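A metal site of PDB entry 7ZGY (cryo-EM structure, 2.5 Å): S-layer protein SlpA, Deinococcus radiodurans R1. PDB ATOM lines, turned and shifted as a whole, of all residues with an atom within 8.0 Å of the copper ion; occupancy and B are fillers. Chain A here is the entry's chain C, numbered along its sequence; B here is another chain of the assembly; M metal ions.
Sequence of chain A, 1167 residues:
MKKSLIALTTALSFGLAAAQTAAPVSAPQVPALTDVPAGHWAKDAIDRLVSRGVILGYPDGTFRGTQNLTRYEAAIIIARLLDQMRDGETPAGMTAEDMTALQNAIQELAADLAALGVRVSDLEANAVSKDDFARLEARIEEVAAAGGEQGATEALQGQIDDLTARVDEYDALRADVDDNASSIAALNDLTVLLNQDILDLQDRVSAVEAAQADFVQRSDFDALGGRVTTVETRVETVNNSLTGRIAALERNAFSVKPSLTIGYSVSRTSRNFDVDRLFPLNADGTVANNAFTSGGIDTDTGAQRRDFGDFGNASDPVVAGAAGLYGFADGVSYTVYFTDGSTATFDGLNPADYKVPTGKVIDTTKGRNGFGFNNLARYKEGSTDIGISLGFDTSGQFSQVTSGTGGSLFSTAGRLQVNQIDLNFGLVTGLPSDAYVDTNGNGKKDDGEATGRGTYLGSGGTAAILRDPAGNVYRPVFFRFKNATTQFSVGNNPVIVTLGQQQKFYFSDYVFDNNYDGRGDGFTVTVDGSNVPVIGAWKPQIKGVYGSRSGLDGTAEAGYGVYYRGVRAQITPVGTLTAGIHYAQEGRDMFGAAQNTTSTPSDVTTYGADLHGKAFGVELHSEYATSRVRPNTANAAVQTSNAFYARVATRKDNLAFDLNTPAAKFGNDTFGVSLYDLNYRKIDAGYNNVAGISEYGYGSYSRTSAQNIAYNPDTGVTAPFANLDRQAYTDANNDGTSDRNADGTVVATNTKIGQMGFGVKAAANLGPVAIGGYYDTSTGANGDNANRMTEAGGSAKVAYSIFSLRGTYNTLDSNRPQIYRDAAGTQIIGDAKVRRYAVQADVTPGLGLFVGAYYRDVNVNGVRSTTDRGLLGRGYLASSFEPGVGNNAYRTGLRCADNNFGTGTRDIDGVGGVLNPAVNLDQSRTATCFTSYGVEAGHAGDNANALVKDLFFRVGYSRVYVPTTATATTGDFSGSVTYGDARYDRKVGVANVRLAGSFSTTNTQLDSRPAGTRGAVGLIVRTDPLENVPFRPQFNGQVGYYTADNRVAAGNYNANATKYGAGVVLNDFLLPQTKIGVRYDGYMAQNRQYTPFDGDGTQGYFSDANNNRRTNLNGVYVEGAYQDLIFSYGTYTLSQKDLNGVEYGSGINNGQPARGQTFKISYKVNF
The backbone NH of Tyr 560 sits at hydrogen-bond distance from the side-chain carboxylate of Asp 553.
O of Val 562 sits at hydrogen-bond distance from N of Arg 549, at 2.9 Å.
OG of Ser 548 lies within hydrogen-bond range of O of Gly 382 of chain B (3.0 Å).
The backbone NH of Ser 548 is in hydrogen-bond range of the backbone carbonyl oxygen of Asp 521.
Ser 548 touches the copper ion (OG to CU, 3.8 Å).
Tyr 560 touches the copper ion (N to CU, 3.8 Å).
Of the 23 residues printed, 7 come within 4 Å of the copper ion.
The copper ion is bound by the backbone carbonyl oxygen (O) of Gly 559, the side-chain carboxylate (OE2) of Glu 381 of chain B, the side-chain carboxylate (OD2) of Asp 553, the backbone carbonyl oxygen (O) of Arg 549 and the backbone carbonyl oxygen (O) of Gly 551.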
ATOM      1  N   ARG A 519     -27.303 -18.231  33.304  1.00  0.00           N
ATOM      2  CA  ARG A 519     -27.802 -19.601  33.356  1.00  0.00           C
ATOM      3  C   ARG A 519     -27.100 -20.539  32.390  1.00  0.00           C
ATOM      4  O   ARG A 519     -26.809 -21.690  32.753  1.00  0.00           O
ATOM      5  CB  ARG A 519     -29.309 -19.630  33.075  1.00  0.00           C
ATOM      6  CG  ARG A 519     -29.988 -20.921  33.490  1.00  0.00           C
ATOM      7  CD  ARG A 519     -31.459 -20.700  33.790  1.00  0.00           C
ATOM      8  NE  ARG A 519     -31.997 -21.732  34.669  1.00  0.00           N
ATOM      9  CZ  ARG A 519     -31.848 -21.760  35.984  1.00  0.00           C
ATOM     10  NH1 ARG A 519     -31.152 -20.826  36.616  1.00  0.00           N
ATOM     11  NH2 ARG A 519     -32.406 -22.745  36.687  1.00  0.00           N
ATOM     12  N   GLY A 520     -26.814 -20.097  31.182  1.00  0.00           N
ATOM     13  CA  GLY A 520     -26.208 -20.980  30.211  1.00  0.00           C
ATOM     14  C   GLY A 520     -25.935 -20.266  28.900  1.00  0.00           C
ATOM     15  O   GLY A 520     -25.924 -19.040  28.836  1.00  0.00           O
ATOM     16  N   ASP A 521     -25.732 -21.066  27.860  1.00  0.00           N
ATOM     17  CA  ASP A 521     -25.340 -20.562  26.556  1.00  0.00           C
ATOM     18  C   ASP A 521     -26.542 -20.489  25.626  1.00  0.00           C
ATOM     19  O   ASP A 521     -27.299 -21.446  25.515  1.00  0.00           O
ATOM     20  CB  ASP A 521     -24.260 -21.449  25.930  1.00  0.00           C
ATOM     21  CG  ASP A 521     -23.044 -21.598  26.820  1.00  0.00           C
ATOM     22  OD1 ASP A 521     -22.949 -20.862  27.827  1.00  0.00           O
ATOM     23  OD2 ASP A 521     -22.174 -22.440  26.509  1.00  0.00           O
ATOM     24  N   GLY A 547     -31.859 -20.812  25.848  1.00  0.00           N
ATOM     25  CA  GLY A 547     -30.505 -21.263  26.122  1.00  0.00           C
ATOM     26  C   GLY A 547     -30.459 -22.677  26.646  1.00  0.00           C
ATOM     27  O   GLY A 547     -31.480 -23.297  26.945  1.00  0.00           O
ATOM     28  N   SER A 548     -29.231 -23.175  26.754  1.00  0.00           N
ATOM     29  CA  SER A 548     -28.922 -24.464  27.336  1.00  0.00           C
ATOM     30  C   SER A 548     -28.157 -24.237  28.641  1.00  0.00           C
ATOM     31  O   SER A 548     -27.145 -23.523  28.648  1.00  0.00           O
ATOM     32  CB  SER A 548     -28.086 -25.309  26.380  1.00  0.00           C
ATOM     33  OG  SER A 548     -27.647 -26.506  26.994  1.00  0.00           O
ATOM     34  N   ARG A 549     -28.641 -24.834  29.730  1.00  0.00           N
ATOM     35  CA  ARG A 549     -28.030 -24.616  31.035  1.00  0.00           C
ATOM     36  C   ARG A 549     -26.578 -25.073  31.028  1.00  0.00           C
ATOM     37  O   ARG A 549     -26.263 -26.200  30.643  1.00  0.00           O
ATOM     38  CB  ARG A 549     -28.805 -25.373  32.109  1.00  0.00           C
ATOM     39  CG  ARG A 549     -29.737 -24.504  32.928  1.00  0.00           C
ATOM     40  CD  ARG A 549     -30.294 -25.282  34.100  1.00  0.00           C
ATOM     41  NE  ARG A 549     -29.347 -25.404  35.198  1.00  0.00           N
ATOM     42  CZ  ARG A 549     -29.642 -25.922  36.385  1.00  0.00           C
ATOM     43  NH1 ARG A 549     -30.846 -26.374  36.659  1.00  0.00           N
ATOM     44  NH2 ARG A 549     -28.699 -25.968  37.319  1.00  0.00           N
ATOM     45  N   SER A 550     -25.691 -24.190  31.492  1.00  0.00           N
ATOM     46  CA  SER A 550     -24.273 -24.465  31.627  1.00  0.00           C
ATOM     47  C   SER A 550     -23.609 -24.840  30.307  1.00  0.00           C
ATOM     48  O   SER A 550     -22.448 -25.258  30.302  1.00  0.00           O
ATOM     49  CB  SER A 550     -24.008 -25.555  32.660  1.00  0.00           C
ATOM     50  OG  SER A 550     -24.592 -25.218  33.904  1.00  0.00           O
ATOM     51  N   GLY A 551     -24.299 -24.679  29.184  1.00  0.00           N
ATOM     52  CA  GLY A 551     -23.735 -25.094  27.916  1.00  0.00           C
ATOM     53  C   GLY A 551     -23.419 -26.570  27.931  1.00  0.00           C
ATOM     54  O   GLY A 551     -24.274 -27.410  28.264  1.00  0.00           O
ATOM     55  N   LEU A 552     -22.191 -26.920  27.567  1.00  0.00           N
ATOM     56  CA  LEU A 552     -21.739 -28.309  27.584  1.00  0.00           C
ATOM     57  C   LEU A 552     -21.315 -28.681  28.998  1.00  0.00           C
ATOM     58  O   LEU A 552     -20.417 -28.058  29.569  1.00  0.00           O
ATOM     59  CB  LEU A 552     -20.595 -28.514  26.603  1.00  0.00           C
ATOM     60  CG  LEU A 552     -20.918 -28.456  25.118  1.00  0.00           C
ATOM     61  CD1 LEU A 552     -19.649 -28.582  24.300  1.00  0.00           C
ATOM     62  CD2 LEU A 552     -21.909 -29.536  24.748  1.00  0.00           C
ATOM     63  N   ASP A 553     -21.965 -29.701  29.559  1.00  0.00           N
ATOM     64  CA  ASP A 553     -21.604 -30.195  30.881  1.00  0.00           C
ATOM     65  C   ASP A 553     -21.812 -31.698  30.919  1.00  0.00           C
ATOM     66  O   ASP A 553     -22.816 -32.214  30.429  1.00  0.00           O
ATOM     67  CB  ASP A 553     -22.432 -29.516  31.977  1.00  0.00           C
ATOM     68  CG  ASP A 553     -23.919 -29.673  31.753  1.00  0.00           C
ATOM     69  OD1 ASP A 553     -24.466 -30.711  32.165  1.00  0.00           O
ATOM     70  OD2 ASP A 553     -24.537 -28.755  31.176  1.00  0.00           O
ATOM     71  N   GLY A 554     -20.847 -32.393  31.505  1.00  0.00           N
ATOM     72  CA  GLY A 554     -20.910 -33.835  31.560  1.00  0.00           C
ATOM     73  C   GLY A 554     -22.037 -34.334  32.445  1.00  0.00           C
ATOM     74  O   GLY A 554     -22.555 -33.628  33.307  1.00  0.00           O
ATOM     75  N   GLU A 557     -24.206 -33.654  36.103  1.00  0.00           N
ATOM     76  CA  GLU A 557     -24.321 -32.228  36.332  1.00  0.00           C
ATOM     77  C   GLU A 557     -25.766 -31.793  36.112  1.00  0.00           C
ATOM     78  O   GLU A 557     -26.469 -32.320  35.244  1.00  0.00           O
ATOM     79  CB  GLU A 557     -23.394 -31.445  35.407  1.00  0.00           C
ATOM     80  CG  GLU A 557     -21.925 -31.734  35.606  1.00  0.00           C
ATOM     81  CD  GLU A 557     -21.031 -30.680  34.985  1.00  0.00           C
ATOM     82  OE1 GLU A 557     -21.322 -29.475  35.166  1.00  0.00           O
ATOM     83  OE2 GLU A 557     -20.031 -31.045  34.333  1.00  0.00           O
ATOM     84  N   ALA A 558     -26.204 -30.816  36.917  1.00  0.00           N
ATOM     85  CA  ALA A 558     -27.592 -30.394  36.877  1.00  0.00           C
ATOM     86  C   ALA A 558     -27.998 -29.810  35.534  1.00  0.00           C
ATOM     87  O   ALA A 558     -29.200 -29.772  35.237  1.00  0.00           O
ATOM     88  CB  ALA A 558     -27.849 -29.361  37.983  1.00  0.00           C
ATOM     89  N   GLY A 559     -27.055 -29.362  34.720  1.00  0.00           N
ATOM     90  CA  GLY A 559     -27.381 -28.703  33.463  1.00  0.00           C
ATOM     91  C   GLY A 559     -27.218 -29.561  32.236  1.00  0.00           C
ATOM     92  O   GLY A 559     -27.100 -29.039  31.119  1.00  0.00           O
ATOM     93  N   TYR A 560     -27.190 -30.882  32.402  1.00  0.00           N
ATOM     94  CA  TYR A 560     -27.021 -31.793  31.272  1.00  0.00           C
ATOM     95  C   TYR A 560     -28.358 -32.013  30.579  1.00  0.00           C
ATOM     96  O   TYR A 560     -29.313 -32.484  31.207  1.00  0.00           O
ATOM     97  CB  TYR A 560     -26.426 -33.116  31.723  1.00  0.00           C
ATOM     98  CG  TYR A 560     -26.178 -34.060  30.572  1.00  0.00           C
ATOM     99  CD1 TYR A 560     -25.039 -33.964  29.796  1.00  0.00           C
ATOM    100  CD2 TYR A 560     -27.113 -35.037  30.233  1.00  0.00           C
ATOM    101  CE1 TYR A 560     -24.817 -34.807  28.736  1.00  0.00           C
ATOM    102  CE2 TYR A 560     -26.901 -35.890  29.176  1.00  0.00           C
ATOM    103  CZ  TYR A 560     -25.749 -35.770  28.426  1.00  0.00           C
ATOM    104  OH  TYR A 560     -25.527 -36.622  27.371  1.00  0.00           O
ATOM    105  N   GLY A 561     -28.424 -31.696  29.290  1.00  0.00           N
ATOM    106  CA  GLY A 561     -29.640 -31.880  28.540  1.00  0.00           C
ATOM    107  C   GLY A 561     -30.807 -31.090  29.079  1.00  0.00           C
ATOM    108  O   GLY A 561     -31.954 -31.532  28.963  1.00  0.00           O
ATOM    109  N   VAL A 562     -30.551 -29.919  29.659  1.00  0.00           N
ATOM    110  CA  VAL A 562     -31.595 -29.073  30.223  1.00  0.00           C
ATOM    111  C   VAL A 562     -31.545 -27.732  29.508  1.00  0.00           C
ATOM    112  O   VAL A 562     -30.483 -27.104  29.409  1.00  0.00           O
ATOM    113  CB  VAL A 562     -31.421 -28.901  31.743  1.00  0.00           C
ATOM    114  CG1 VAL A 562     -30.118 -28.230  32.057  1.00  0.00           C
ATOM    115  CG2 VAL A 562     -32.575 -28.096  32.311  1.00  0.00           C
ATOM    116  N   TYR A 563     -32.699 -27.295  29.004  1.00  0.00           N
ATOM    117  CA  TYR A 563     -32.816 -26.089  28.211  1.00  0.00           C
ATOM    118  C   TYR A 563     -33.907 -25.203  28.789  1.00  0.00           C
ATOM    119  O   TYR A 563     -34.932 -25.711  29.271  1.00  0.00           O
ATOM    120  CB  TYR A 563     -33.111 -26.411  26.748  1.00  0.00           C
ATOM    121  CG  TYR A 563     -32.033 -27.240  26.104  1.00  0.00           C
ATOM    122  CD1 TYR A 563     -31.994 -28.610  26.285  1.00  0.00           C
ATOM    123  CD2 TYR A 563     -31.039 -26.658  25.339  1.00  0.00           C
ATOM    124  CE1 TYR A 563     -31.007 -29.370  25.711  1.00  0.00           C
ATOM    125  CE2 TYR A 563     -30.042 -27.418  24.768  1.00  0.00           C
ATOM    126  CZ  TYR A 563     -30.037 -28.773  24.956  1.00  0.00           C
ATOM    127  OH  TYR A 563     -29.050 -29.542  24.387  1.00  0.00           O
ATOM    128  N   ASN A 596     -29.028 -38.285  33.056  1.00  0.00           N
ATOM    129  CA  ASN A 596     -28.692 -36.991  33.641  1.00  0.00           C
ATOM    130  C   ASN A 596     -28.456 -37.141  35.140  1.00  0.00           C
ATOM    131  O   ASN A 596     -27.688 -36.381  35.738  1.00  0.00           O
ATOM    132  CB  ASN A 596     -29.783 -35.952  33.392  1.00  0.00           C
ATOM    133  CG  ASN A 596     -29.464 -34.615  34.042  1.00  0.00           C
ATOM    134  OD1 ASN A 596     -28.311 -34.315  34.344  1.00  0.00           O
ATOM    135  ND2 ASN A 596     -30.497 -33.795  34.257  1.00  0.00           N
ATOM    136  N   TYR B 379     -25.859 -37.065  20.349  1.00  0.00           N
ATOM    137  CA  TYR B 379     -26.314 -35.846  20.985  1.00  0.00           C
ATOM    138  C   TYR B 379     -25.224 -34.790  20.922  1.00  0.00           C
ATOM    139  O   TYR B 379     -24.055 -35.068  21.181  1.00  0.00           O
ATOM    140  CB  TYR B 379     -26.698 -36.094  22.451  1.00  0.00           C
ATOM    141  CG  TYR B 379     -27.342 -34.910  23.127  1.00  0.00           C
ATOM    142  CD1 TYR B 379     -28.280 -34.127  22.471  1.00  0.00           C
ATOM    143  CD2 TYR B 379     -27.019 -34.572  24.441  1.00  0.00           C
ATOM    144  CE1 TYR B 379     -28.873 -33.051  23.087  1.00  0.00           C
ATOM    145  CE2 TYR B 379     -27.612 -33.496  25.058  1.00  0.00           C
ATOM    146  CZ  TYR B 379     -28.534 -32.743  24.386  1.00  0.00           C
ATOM    147  OH  TYR B 379     -29.134 -31.663  24.987  1.00  0.00           O
ATOM    148  N   GLU B 381     -24.958 -31.468  22.899  1.00  0.00           N
ATOM    149  CA  GLU B 381     -25.559 -30.612  23.907  1.00  0.00           C
ATOM    150  C   GLU B 381     -25.389 -29.157  23.518  1.00  0.00           C
ATOM    151  O   GLU B 381     -24.298 -28.710  23.140  1.00  0.00           O
ATOM    152  CB  GLU B 381     -24.931 -30.864  25.277  1.00  0.00           C
ATOM    153  CG  GLU B 381     -25.837 -30.500  26.430  1.00  0.00           C
ATOM    154  CD  GLU B 381     -25.117 -30.520  27.753  1.00  0.00           C
ATOM    155  OE1 GLU B 381     -24.137 -31.272  27.880  1.00  0.00           O
ATOM    156  OE2 GLU B 381     -25.526 -29.769  28.665  1.00  0.00           O
ATOM    157  N   GLY B 382     -26.475 -28.396  23.612  1.00  0.00           N
ATOM    158  CA  GLY B 382     -26.462 -27.021  23.167  1.00  0.00           C
ATOM    159  C   GLY B 382     -25.413 -26.183  23.863  1.00  0.00           C
ATOM    160  O   GLY B 382     -25.356 -26.138  25.097  1.00  0.00           O
ATOM    161  N   SER B 383     -24.568 -25.506  23.084  1.00  0.00           N
ATOM    162  CA  SER B 383     -23.581 -24.606  23.655  1.00  0.00           C
ATOM    163  C   SER B 383     -23.196 -23.568  22.622  1.00  0.00           C
ATOM    164  O   SER B 383     -23.378 -23.768  21.411  1.00  0.00           O
ATOM    165  CB  SER B 383     -22.343 -25.358  24.129  1.00  0.00           C
ATOM    166  OG  SER B 383     -21.539 -25.758  23.037  1.00  0.00           O
HETATM  167 CU    CU M   1     -25.977 -28.307  29.845  1.00  0.00          CU
